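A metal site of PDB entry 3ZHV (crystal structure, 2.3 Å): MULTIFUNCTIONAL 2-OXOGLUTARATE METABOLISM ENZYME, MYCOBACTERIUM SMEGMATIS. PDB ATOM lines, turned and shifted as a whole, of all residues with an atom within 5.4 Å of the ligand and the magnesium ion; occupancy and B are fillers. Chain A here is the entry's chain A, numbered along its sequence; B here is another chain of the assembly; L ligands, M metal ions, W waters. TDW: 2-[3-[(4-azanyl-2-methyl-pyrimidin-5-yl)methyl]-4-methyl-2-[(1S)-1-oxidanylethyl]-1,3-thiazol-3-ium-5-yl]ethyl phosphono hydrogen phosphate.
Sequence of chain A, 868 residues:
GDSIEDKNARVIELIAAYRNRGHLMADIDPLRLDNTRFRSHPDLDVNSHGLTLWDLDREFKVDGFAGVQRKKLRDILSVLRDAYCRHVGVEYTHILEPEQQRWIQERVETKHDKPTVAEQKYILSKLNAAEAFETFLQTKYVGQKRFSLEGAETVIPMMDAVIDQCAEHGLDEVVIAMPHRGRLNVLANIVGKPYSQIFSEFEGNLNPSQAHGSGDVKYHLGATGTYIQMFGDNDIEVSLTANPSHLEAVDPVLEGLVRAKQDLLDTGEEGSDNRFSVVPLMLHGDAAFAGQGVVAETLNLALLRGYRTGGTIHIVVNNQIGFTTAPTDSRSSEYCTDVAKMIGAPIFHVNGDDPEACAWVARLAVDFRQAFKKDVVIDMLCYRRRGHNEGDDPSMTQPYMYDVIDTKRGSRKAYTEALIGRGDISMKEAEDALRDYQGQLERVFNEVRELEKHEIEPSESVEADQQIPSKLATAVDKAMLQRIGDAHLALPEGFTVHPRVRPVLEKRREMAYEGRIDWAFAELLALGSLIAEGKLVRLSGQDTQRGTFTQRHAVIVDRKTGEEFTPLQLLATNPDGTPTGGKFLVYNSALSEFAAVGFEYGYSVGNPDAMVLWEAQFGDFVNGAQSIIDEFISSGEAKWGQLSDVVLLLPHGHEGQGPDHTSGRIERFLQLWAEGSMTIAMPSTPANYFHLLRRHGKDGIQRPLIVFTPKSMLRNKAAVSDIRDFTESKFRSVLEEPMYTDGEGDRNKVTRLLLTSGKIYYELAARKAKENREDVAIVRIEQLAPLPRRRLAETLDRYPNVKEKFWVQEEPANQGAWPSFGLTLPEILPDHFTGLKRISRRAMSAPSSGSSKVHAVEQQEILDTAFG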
ATOM      1  N   HIS A 180      16.775 -11.079   6.466  1.00  0.00           N
ATOM      2  CA  HIS A 180      15.361 -11.395   6.719  1.00  0.00           C
ATOM      3  C   HIS A 180      14.339 -10.844   5.682  1.00  0.00           C
ATOM      4  O   HIS A 180      13.297 -11.475   5.499  1.00  0.00           O
ATOM      5  CB  HIS A 180      14.956 -10.943   8.153  1.00  0.00           C
ATOM      6  CG  HIS A 180      15.097  -9.463   8.359  1.00  0.00           C
ATOM      7  ND1 HIS A 180      16.274  -8.902   8.844  1.00  0.00           N
ATOM      8  CD2 HIS A 180      14.226  -8.466   8.090  1.00  0.00           C
ATOM      9  CE1 HIS A 180      16.082  -7.599   8.876  1.00  0.00           C
ATOM     10  NE2 HIS A 180      14.863  -7.278   8.416  1.00  0.00           N
ATOM     11  N   ARG A 181      14.588  -9.690   5.015  1.00  0.00           N
ATOM     12  CA  ARG A 181      13.650  -9.057   4.052  1.00  0.00           C
ATOM     13  C   ARG A 181      13.279  -9.967   2.837  1.00  0.00           C
ATOM     14  O   ARG A 181      14.112 -10.253   1.971  1.00  0.00           O
ATOM     15  CB  ARG A 181      14.191  -7.694   3.550  1.00  0.00           C
ATOM     16  CG  ARG A 181      13.103  -6.851   2.856  1.00  0.00           C
ATOM     17  CD  ARG A 181      13.569  -5.466   2.428  1.00  0.00           C
ATOM     18  NE  ARG A 181      14.052  -4.650   3.553  1.00  0.00           N
ATOM     19  CZ  ARG A 181      13.259  -4.004   4.405  1.00  0.00           C
ATOM     20  NH1 ARG A 181      11.937  -4.046   4.269  1.00  0.00           N
ATOM     21  NH2 ARG A 181      13.779  -3.285   5.400  1.00  0.00           N
ATOM     22  N   SER A 245      20.622 -12.288  13.086  1.00  0.00           N
ATOM     23  CA  SER A 245      20.186 -10.962  12.609  1.00  0.00           C
ATOM     24  C   SER A 245      21.390 -10.136  12.163  1.00  0.00           C
ATOM     25  O   SER A 245      21.213  -9.167  11.453  1.00  0.00           O
ATOM     26  CB  SER A 245      19.419 -10.205  13.685  1.00  0.00           C
ATOM     27  OG  SER A 245      18.204 -10.841  14.038  1.00  0.00           O
ATOM     28  N   HIS A 246      22.618 -10.516  12.573  1.00  0.00           N
ATOM     29  CA  HIS A 246      23.897  -9.875  12.202  1.00  0.00           C
ATOM     30  C   HIS A 246      24.082  -9.948  10.709  1.00  0.00           C
ATOM     31  O   HIS A 246      24.425 -11.008  10.175  1.00  0.00           O
ATOM     32  CB  HIS A 246      25.074 -10.530  12.944  1.00  0.00           C
ATOM     33  CG  HIS A 246      25.079 -10.273  14.417  1.00  0.00           C
ATOM     34  ND1 HIS A 246      23.995 -10.611  15.204  1.00  0.00           N
ATOM     35  CD2 HIS A 246      26.033  -9.714  15.190  1.00  0.00           C
ATOM     36  CE1 HIS A 246      24.319 -10.234  16.428  1.00  0.00           C
ATOM     37  NE2 HIS A 246      25.537  -9.691  16.468  1.00  0.00           N
ATOM     38  N   LEU A 247      23.801  -8.826  10.031  1.00  0.00           N
ATOM     39  CA  LEU A 247      23.839  -8.717   8.575  1.00  0.00           C
ATOM     40  C   LEU A 247      25.246  -9.003   8.055  1.00  0.00           C
ATOM     41  O   LEU A 247      26.223  -8.537   8.618  1.00  0.00           O
ATOM     42  CB  LEU A 247      23.338  -7.335   8.094  1.00  0.00           C
ATOM     43  CG  LEU A 247      21.907  -6.926   8.525  1.00  0.00           C
ATOM     44  CD1 LEU A 247      21.652  -5.445   8.342  1.00  0.00           C
ATOM     45  CD2 LEU A 247      20.841  -7.751   7.800  1.00  0.00           C
ATOM     46  N   GLY A 285      21.723  -6.383   1.509  1.00  0.00           N
ATOM     47  CA  GLY A 285      21.129  -5.054   1.608  1.00  0.00           C
ATOM     48  C   GLY A 285      22.211  -4.067   1.216  1.00  0.00           C
ATOM     49  O   GLY A 285      23.400  -4.351   1.392  1.00  0.00           O
ATOM     50  N   ASP A 286      21.831  -2.908   0.681  1.00  0.00           N
ATOM     51  CA  ASP A 286      22.784  -1.916   0.211  1.00  0.00           C
ATOM     52  C   ASP A 286      23.625  -1.291   1.337  1.00  0.00           C
ATOM     53  O   ASP A 286      24.812  -1.052   1.099  1.00  0.00           O
ATOM     54  CB  ASP A 286      22.085  -0.796  -0.603  1.00  0.00           C
ATOM     55  CG  ASP A 286      20.953  -0.074   0.120  1.00  0.00           C
ATOM     56  OD1 ASP A 286      19.980  -0.757   0.561  1.00  0.00           O
ATOM     57  OD2 ASP A 286      21.017   1.167   0.221  1.00  0.00           O
ATOM     58  N   ALA A 287      23.043  -1.019   2.516  1.00  0.00           N
ATOM     59  CA  ALA A 287      23.856  -0.376   3.580  1.00  0.00           C
ATOM     60  C   ALA A 287      24.854  -1.377   4.174  1.00  0.00           C
ATOM     61  O   ALA A 287      26.017  -1.038   4.366  1.00  0.00           O
ATOM     62  CB  ALA A 287      22.953   0.231   4.679  1.00  0.00           C
ATOM     63  N   ALA A 288      24.403  -2.632   4.371  1.00  0.00           N
ATOM     64  CA  ALA A 288      25.217  -3.704   4.954  1.00  0.00           C
ATOM     65  C   ALA A 288      26.366  -4.139   4.017  1.00  0.00           C
ATOM     66  O   ALA A 288      27.472  -4.358   4.481  1.00  0.00           O
ATOM     67  CB  ALA A 288      24.315  -4.901   5.283  1.00  0.00           C
ATOM     68  N   PHE A 289      26.086  -4.230   2.702  1.00  0.00           N
ATOM     69  CA  PHE A 289      27.072  -4.641   1.718  1.00  0.00           C
ATOM     70  C   PHE A 289      28.274  -3.677   1.675  1.00  0.00           C
ATOM     71  O   PHE A 289      29.401  -4.134   1.495  1.00  0.00           O
ATOM     72  CB  PHE A 289      26.446  -4.769   0.306  1.00  0.00           C
ATOM     73  CG  PHE A 289      27.293  -5.585  -0.649  1.00  0.00           C
ATOM     74  CD1 PHE A 289      27.448  -6.955  -0.458  1.00  0.00           C
ATOM     75  CD2 PHE A 289      27.949  -4.988  -1.707  1.00  0.00           C
ATOM     76  CE1 PHE A 289      28.223  -7.711  -1.337  1.00  0.00           C
ATOM     77  CE2 PHE A 289      28.715  -5.740  -2.585  1.00  0.00           C
ATOM     78  CZ  PHE A 289      28.852  -7.101  -2.407  1.00  0.00           C
ATOM     79  N   GLN A 292      29.903  -3.539   6.075  1.00  0.00           N
ATOM     80  CA  GLN A 292      30.378  -4.691   6.842  1.00  0.00           C
ATOM     81  C   GLN A 292      31.688  -5.219   6.261  1.00  0.00           C
ATOM     82  O   GLN A 292      31.732  -5.579   5.093  1.00  0.00           O
ATOM     83  CB  GLN A 292      29.285  -5.796   6.893  1.00  0.00           C
ATOM     84  CG  GLN A 292      28.108  -5.471   7.818  1.00  0.00           C
ATOM     85  CD  GLN A 292      28.512  -5.376   9.278  1.00  0.00           C
ATOM     86  OE1 GLN A 292      29.046  -6.306   9.846  1.00  0.00           O
ATOM     87  NE2 GLN A 292      28.319  -4.231   9.905  1.00  0.00           N
ATOM     88  N   VAL A 317      19.837  -6.111  -2.842  1.00  0.00           N
ATOM     89  CA  VAL A 317      18.518  -5.515  -2.848  1.00  0.00           C
ATOM     90  C   VAL A 317      18.753  -4.061  -2.427  1.00  0.00           C
ATOM     91  O   VAL A 317      18.754  -3.727  -1.220  1.00  0.00           O
ATOM     92  CB  VAL A 317      17.489  -6.281  -1.972  1.00  0.00           C
ATOM     93  CG1 VAL A 317      16.106  -5.623  -2.010  1.00  0.00           C
ATOM     94  CG2 VAL A 317      17.397  -7.751  -2.405  1.00  0.00           C
ATOM     95  N   ASN A 319      17.579  -0.868  -2.042  1.00  0.00           N
ATOM     96  CA  ASN A 319      16.388  -0.044  -1.880  1.00  0.00           C
ATOM     97  C   ASN A 319      16.757   1.403  -1.497  1.00  0.00           C
ATOM     98  O   ASN A 319      15.886   2.176  -1.099  1.00  0.00           O
ATOM     99  CB  ASN A 319      15.414  -0.666  -0.887  1.00  0.00           C
ATOM    100  CG  ASN A 319      15.989  -0.982   0.462  1.00  0.00           C
ATOM    101  OD1 ASN A 319      17.015  -0.422   0.889  1.00  0.00           O
ATOM    102  ND2 ASN A 319      15.307  -1.889   1.161  1.00  0.00           N
ATOM    103  N   GLN A 320      18.058   1.748  -1.647  1.00  0.00           N
ATOM    104  CA  GLN A 320      18.655   3.084  -1.513  1.00  0.00           C
ATOM    105  C   GLN A 320      18.374   3.718  -0.153  1.00  0.00           C
ATOM    106  O   GLN A 320      18.207   4.931  -0.040  1.00  0.00           O
ATOM    107  CB  GLN A 320      18.151   4.011  -2.662  1.00  0.00           C
ATOM    108  CG  GLN A 320      18.193   3.364  -4.065  1.00  0.00           C
ATOM    109  CD  GLN A 320      17.594   4.221  -5.140  1.00  0.00           C
ATOM    110  OE1 GLN A 320      18.111   5.289  -5.481  1.00  0.00           O
ATOM    111  NE2 GLN A 320      16.512   3.765  -5.742  1.00  0.00           N
ATOM    112  N   ILE A 321      18.286   2.870   0.879  1.00  0.00           N
ATOM    113  CA  ILE A 321      18.025   3.283   2.267  1.00  0.00           C
ATOM    114  C   ILE A 321      18.483   2.157   3.199  1.00  0.00           C
ATOM    115  O   ILE A 321      18.546   0.981   2.784  1.00  0.00           O
ATOM    116  CB  ILE A 321      16.516   3.701   2.500  1.00  0.00           C
ATOM    117  CG1 ILE A 321      16.342   4.494   3.815  1.00  0.00           C
ATOM    118  CG2 ILE A 321      15.513   2.511   2.331  1.00  0.00           C
ATOM    119  CD1 ILE A 321      15.073   5.279   3.936  1.00  0.00           C
ATOM    120  N   GLY A 322      18.874   2.546   4.401  1.00  0.00           N
ATOM    121  CA  GLY A 322      19.296   1.665   5.484  1.00  0.00           C
ATOM    122  C   GLY A 322      18.644   2.153   6.756  1.00  0.00           C
ATOM    123  O   GLY A 322      19.198   3.036   7.427  1.00  0.00           O
ATOM    124  N   PHE A 323      17.424   1.662   7.063  1.00  0.00           N
ATOM    125  CA  PHE A 323      16.566   2.061   8.188  1.00  0.00           C
ATOM    126  C   PHE A 323      16.157   3.555   7.985  1.00  0.00           C
ATOM    127  O   PHE A 323      15.227   3.825   7.228  1.00  0.00           O
ATOM    128  CB  PHE A 323      17.235   1.767   9.560  1.00  0.00           C
ATOM    129  CG  PHE A 323      16.330   1.658  10.773  1.00  0.00           C
ATOM    130  CD1 PHE A 323      15.209   2.474  10.900  1.00  0.00           C
ATOM    131  CD2 PHE A 323      16.613   0.752  11.786  1.00  0.00           C
ATOM    132  CE1 PHE A 323      14.359   2.351  12.003  1.00  0.00           C
ATOM    133  CE2 PHE A 323      15.752   0.627  12.880  1.00  0.00           C
ATOM    134  CZ  PHE A 323      14.655   1.449  13.010  1.00  0.00           C
ATOM    135  N   ARG A 384      12.020   0.774  -0.781  1.00  0.00           N
ATOM    136  CA  ARG A 384      11.362   0.165   0.353  1.00  0.00           C
ATOM    137  C   ARG A 384      10.050   0.885   0.486  1.00  0.00           C
ATOM    138  O   ARG A 384      10.039   2.027   0.931  1.00  0.00           O
ATOM    139  CB  ARG A 384      12.235   0.289   1.616  1.00  0.00           C
ATOM    140  CG  ARG A 384      11.860  -0.691   2.719  1.00  0.00           C
ATOM    141  CD  ARG A 384      12.477  -0.211   4.004  1.00  0.00           C
ATOM    142  NE  ARG A 384      11.930   1.105   4.335  1.00  0.00           N
ATOM    143  CZ  ARG A 384      12.530   2.021   5.082  1.00  0.00           C
ATOM    144  NH1 ARG A 384      13.731   1.796   5.586  1.00  0.00           N
ATOM    145  NH2 ARG A 384      11.940   3.194   5.305  1.00  0.00           N
ATOM    146  N   HIS A 388      10.589   1.207   7.855  1.00  0.00           N
ATOM    147  CA  HIS A 388      11.478   0.128   8.236  1.00  0.00           C
ATOM    148  C   HIS A 388      10.756  -0.887   9.148  1.00  0.00           C
ATOM    149  O   HIS A 388      10.980  -2.082   8.976  1.00  0.00           O
ATOM    150  CB  HIS A 388      12.752   0.644   8.912  1.00  0.00           C
ATOM    151  CG  HIS A 388      13.851  -0.376   8.953  1.00  0.00           C
ATOM    152  ND1 HIS A 388      14.550  -0.742   7.800  1.00  0.00           N
ATOM    153  CD2 HIS A 388      14.294  -1.127   9.981  1.00  0.00           C
ATOM    154  CE1 HIS A 388      15.416  -1.674   8.186  1.00  0.00           C
ATOM    155  NE2 HIS A 388      15.295  -1.945   9.484  1.00  0.00           N
ATOM    156  N   GLN B 542      24.230   3.946  14.430  1.00  0.00           N
ATOM    157  CA  GLN B 542      23.239   3.642  13.403  1.00  0.00           C
ATOM    158  C   GLN B 542      21.892   4.306  13.717  1.00  0.00           C
ATOM    159  O   GLN B 542      21.307   4.065  14.789  1.00  0.00           O
ATOM    160  CB  GLN B 542      23.097   2.123  13.232  1.00  0.00           C
ATOM    161  CG  GLN B 542      24.241   1.508  12.433  1.00  0.00           C
ATOM    162  CD  GLN B 542      24.577   0.116  12.853  1.00  0.00           C
ATOM    163  OE1 GLN B 542      23.738  -0.643  13.340  1.00  0.00           O
ATOM    164  NE2 GLN B 542      25.823  -0.274  12.665  1.00  0.00           N
ATOM    165  N   ASP B 543      21.460   5.227  12.824  1.00  0.00           N
ATOM    166  CA  ASP B 543      20.206   5.999  12.914  1.00  0.00           C
ATOM    167  C   ASP B 543      20.083   6.786  14.244  1.00  0.00           C
ATOM    168  O   ASP B 543      18.991   7.036  14.734  1.00  0.00           O
ATOM    169  CB  ASP B 543      18.991   5.056  12.714  1.00  0.00           C
ATOM    170  CG  ASP B 543      19.141   4.152  11.502  1.00  0.00           C
ATOM    171  OD1 ASP B 543      18.990   4.659  10.357  1.00  0.00           O
ATOM    172  OD2 ASP B 543      19.543   2.972  11.691  1.00  0.00           O
ATOM    173  N   LEU B 591      26.888   1.335   8.236  1.00  0.00           N
ATOM    174  CA  LEU B 591      26.498   0.085   8.874  1.00  0.00           C
ATOM    175  C   LEU B 591      27.768  -0.717   9.244  1.00  0.00           C
ATOM    176  O   LEU B 591      28.061  -1.764   8.667  1.00  0.00           O
ATOM    177  CB  LEU B 591      25.549  -0.721   7.970  1.00  0.00           C
ATOM    178  CG  LEU B 591      24.506  -1.569   8.673  1.00  0.00           C
ATOM    179  CD1 LEU B 591      23.381  -1.904   7.742  1.00  0.00           C
ATOM    180  CD2 LEU B 591      25.113  -2.872   9.272  1.00  0.00           C
ATOM    181  N   GLU B 593      30.404  -1.656  12.882  1.00  0.00           N
ATOM    182  CA  GLU B 593      30.565  -1.646  14.318  1.00  0.00           C
ATOM    183  C   GLU B 593      32.030  -1.487  14.612  1.00  0.00           C
ATOM    184  O   GLU B 593      32.385  -0.535  15.291  1.00  0.00           O
ATOM    185  CB  GLU B 593      29.975  -2.895  14.991  1.00  0.00           C
ATOM    186  CG  GLU B 593      28.454  -2.861  15.081  1.00  0.00           C
ATOM    187  CD  GLU B 593      27.717  -3.265  13.817  1.00  0.00           C
ATOM    188  OE1 GLU B 593      28.259  -4.058  13.013  1.00  0.00           O
ATOM    189  OE2 GLU B 593      26.593  -2.759  13.616  1.00  0.00           O
ATOM    190  N   GLN B 617      22.884  -0.072  17.583  1.00  0.00           N
ATOM    191  CA  GLN B 617      21.496  -0.121  17.172  1.00  0.00           C
ATOM    192  C   GLN B 617      20.713  -0.872  18.253  1.00  0.00           C
ATOM    193  O   GLN B 617      19.673  -0.411  18.751  1.00  0.00           O
ATOM    194  CB  GLN B 617      21.354  -0.780  15.773  1.00  0.00           C
ATOM    195  CG  GLN B 617      19.903  -0.789  15.296  1.00  0.00           C
ATOM    196  CD  GLN B 617      19.689   0.062  14.099  1.00  0.00           C
ATOM    197  OE1 GLN B 617      19.674  -0.411  12.974  1.00  0.00           O
ATOM    198  NE2 GLN B 617      19.454   1.344  14.305  1.00  0.00           N
ATOM    199  N   PHE B 618      21.285  -2.010  18.649  1.00  0.00           N
ATOM    200  CA  PHE B 618      20.923  -2.921  19.733  1.00  0.00           C
ATOM    201  C   PHE B 618      22.260  -3.339  20.292  1.00  0.00           C
ATOM    202  O   PHE B 618      23.196  -3.488  19.499  1.00  0.00           O
ATOM    203  CB  PHE B 618      20.113  -4.128  19.212  1.00  0.00           C
ATOM    204  CG  PHE B 618      18.666  -3.811  18.901  1.00  0.00           C
ATOM    205  CD1 PHE B 618      18.314  -3.291  17.655  1.00  0.00           C
ATOM    206  CD2 PHE B 618      17.665  -4.074  19.825  1.00  0.00           C
ATOM    207  CE1 PHE B 618      16.971  -3.008  17.362  1.00  0.00           C
ATOM    208  CE2 PHE B 618      16.318  -3.803  19.529  1.00  0.00           C
ATOM    209  CZ  PHE B 618      15.987  -3.257  18.298  1.00  0.00           C
ATOM    210  N   PHE B 621      24.798  -6.165  18.639  1.00  0.00           N
ATOM    211  CA  PHE B 621      25.660  -6.029  17.467  1.00  0.00           C
ATOM    212  C   PHE B 621      27.041  -5.475  17.815  1.00  0.00           C
ATOM    213  O   PHE B 621      27.905  -5.459  16.934  1.00  0.00           O
ATOM    214  CB  PHE B 621      24.972  -5.184  16.385  1.00  0.00           C
ATOM    215  CG  PHE B 621      23.630  -5.740  15.994  1.00  0.00           C
ATOM    216  CD1 PHE B 621      23.528  -6.973  15.369  1.00  0.00           C
ATOM    217  CD2 PHE B 621      22.463  -5.043  16.259  1.00  0.00           C
ATOM    218  CE1 PHE B 621      22.280  -7.511  15.017  1.00  0.00           C
ATOM    219  CE2 PHE B 621      21.204  -5.581  15.920  1.00  0.00           C
ATOM    220  CZ  PHE B 621      21.126  -6.804  15.284  1.00  0.00           C
ATOM    221  N   HIS B 661      18.298  -9.202  19.553  1.00  0.00           N
ATOM    222  CA  HIS B 661      17.612  -7.951  19.906  1.00  0.00           C
ATOM    223  C   HIS B 661      17.250  -7.993  21.400  1.00  0.00           C
ATOM    224  O   HIS B 661      16.175  -7.530  21.788  1.00  0.00           O
ATOM    225  CB  HIS B 661      16.369  -7.747  19.024  1.00  0.00           C
ATOM    226  CG  HIS B 661      16.688  -7.624  17.577  1.00  0.00           C
ATOM    227  ND1 HIS B 661      16.673  -8.735  16.745  1.00  0.00           N
ATOM    228  CD2 HIS B 661      17.080  -6.542  16.870  1.00  0.00           C
ATOM    229  CE1 HIS B 661      17.037  -8.295  15.564  1.00  0.00           C
ATOM    230  NE2 HIS B 661      17.295  -6.977  15.576  1.00  0.00           N
HETATM  231  S1  TDW L   1      18.273  -3.460   9.742  1.00  0.00           S
HETATM  232  C2  TDW L   1      18.817  -3.883  11.252  1.00  0.00           C
HETATM  233  N3  TDW L   1      20.108  -3.284  11.607  1.00  0.00           N
HETATM  234  C4  TDW L   1      20.458  -2.383  10.578  1.00  0.00           C
HETATM  235  C5  TDW L   1      19.528  -2.415   9.487  1.00  0.00           C
HETATM  236  C6  TDW L   1      19.600  -1.531   8.275  1.00  0.00           C
HETATM  237  C7  TDW L   1      19.794  -2.433   7.087  1.00  0.00           C
HETATM  238  O7  TDW L   1      20.130  -1.706   5.879  1.00  0.00           O
HETATM  239  PA  TDW L   1      20.359  -2.550   4.532  1.00  0.00           P
HETATM  240  PB  TDW L   1      17.393  -3.002   4.193  1.00  0.00           P
HETATM  241  N1' TDW L   1      24.581  -4.369  12.421  1.00  0.00           N
HETATM  242  O1A TDW L   1      21.517  -3.480   4.473  1.00  0.00           O
HETATM  243  O1B TDW L   1      17.094  -4.190   3.272  1.00  0.00           O
HETATM  244  C2' TDW L   1      24.508  -5.629  11.980  1.00  0.00           C
HETATM  245  C27 TDW L   1      17.938  -4.570  12.307  1.00  0.00           C
HETATM  246  O28 TDW L   1      18.538  -5.632  13.028  1.00  0.00           O
HETATM  247  C29 TDW L   1      17.347  -3.567  13.260  1.00  0.00           C
HETATM  248  O2A TDW L   1      20.305  -1.410   3.498  1.00  0.00           O
HETATM  249  O2B TDW L   1      16.849  -3.101   5.621  1.00  0.00           O
HETATM  250  N3' TDW L   1      23.381  -6.321  11.793  1.00  0.00           N
HETATM  251  O3A TDW L   1      18.917  -3.090   4.403  1.00  0.00           O
HETATM  252  O3B TDW L   1      17.090  -1.613   3.556  1.00  0.00           O
HETATM  253  C4' TDW L   1      22.205  -5.710  12.073  1.00  0.00           C
HETATM  254  N4' TDW L   1      21.098  -6.440  11.914  1.00  0.00           N
HETATM  255  C5' TDW L   1      22.180  -4.368  12.536  1.00  0.00           C
HETATM  256  C6' TDW L   1      23.410  -3.774  12.697  1.00  0.00           C
HETATM  257  C7' TDW L   1      20.907  -3.581  12.810  1.00  0.00           C
HETATM  258  CM2 TDW L   1      25.794  -6.315  11.658  1.00  0.00           C
HETATM  259  CM4 TDW L   1      21.578  -1.402  10.732  1.00  0.00           C
HETATM  260 MG    MG M   1      18.604  -0.900   2.268  1.00  0.00          MG
HETATM  261  O   HOH W   1      20.719  -6.095   4.914  1.00  0.00           O
HETATM  262  O   HOH W   2      18.468  -2.770   1.250  1.00  0.00           O
HETATM  263  O   HOH W   3      18.128  -6.527   3.361  1.00  0.00           O
HETATM  264  O   HOH W   4      15.953  -0.202   5.403  1.00  0.00           O
HETATM  265  O   HOH W   5      15.539  -6.361  12.971  1.00  0.00           O
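The backbone carbonyl oxygen of Gln 542 of chain B lies within hydrogen-bond range of the side-chain amide nitrogen of Gln 617 of chain B (3.3 Å). NE2 of Gln 617 of chain B sits at hydrogen-bond distance from OD2 of Asp 543 of chain B (3.1 Å). The side-chain carboxylate (OE2) of Glu 593 of chain B is in hydrogen-bond range of the side-chain amide nitrogen (NE2) of Gln 542 of chain B (2.8 Å). OE1 of Glu 593 of chain B lies within hydrogen-bond range of NE2 of Gln 292 (3.1 Å). ND1 of His 388 lies within hydrogen-bond range of NH1 of Arg 384, 3.5 Å away. O of Leu 591 of chain B lies within hydrogen-bond range of NE2 of Gln 292.
N3' of the ligand sits at hydrogen-bond distance from N of Leu 247 (3.1 Å). NE2 of His 661 of chain B is in hydrogen-bond range of O28 of the ligand (3.1 Å). The guanidinium group (NH2) of Arg 181 is in salt-bridge range of an oxygen (O2B) of the ligand (3.1 Å). N of Ala 288 lies within hydrogen-bond range of O1A of the ligand, at 3.0 Å. The side-chain carboxylate of Glu 593 of chain B is in hydrogen-bond range of a nitrogen (N1') of the ligand, at 2.8 Å. A sulfur (S1) of the ligand lies close to a ring nitrogen (NE2) of His 388, 3.4 Å away. A nitrogen (N4') of the ligand lies within hydrogen-bond range of the backbone carbonyl oxygen of Ser 245. N of Ala 287 lies within hydrogen-bond range of O1A of the ligand.
A nitrogen (N3) of the ligand sits close to the side-chain amide oxygen (OE1) of Gln 617 of chain B, 3.2 Å away. Residues that only touch the ligand: Gln 542 of chain B, Gly 285, Phe 621 of chain B, Gly 322, Leu 591 of chain B, His 246 and Gln 292. 19 residues have an atom within 4 Å of the ligand: Arg 181, Ser 245, His 246, Leu 247, Gly 285, Asp 286, Ala 287, Ala 288, Gln 292, Asn 319, Ile 321, Gly 322, His 388, Gln 542 of chain B, Leu 591 of chain B, Glu 593 of chain B, Gln 617 of chain B, Phe 621 of chain B and His 661 of chain B. The nearest printed residue that does not touch the ligand is Phe 323 (4.05 Å).
The magnesium ion is bound by O of Ile 321 (2.0 Å), O3B of the ligand (2.1 Å), water W2 (2.1 Å), OD1 of Asn 319 (2.2 Å), O2A of the ligand (2.2 Å) and OD1 of Asp 286 (2.2 Å).
Within 4 Å of the magnesium ion: Asp 286, Asn 319 and Ile 321.
Water W2 lies within hydrogen-bond range of the backbone carbonyl oxygen of Val 317 (2.7 Å), an oxygen (O1B) of the ligand (2.8 Å), the side-chain amide nitrogen of Asn 319 (3.3 Å) and the backbone NH of Asp 286 (3.4 Å). Water W4 lies within hydrogen-bond range of ND1 of His 388 (2.8 Å), N of Phe 323 (2.9 Å), NH1 of Arg 384 (3.0 Å) and O2B of the ligand (3.0 Å). Water W5 bridges an oxygen (O28) of the ligand and a ring nitrogen (NE2) of His 661 of chain B.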
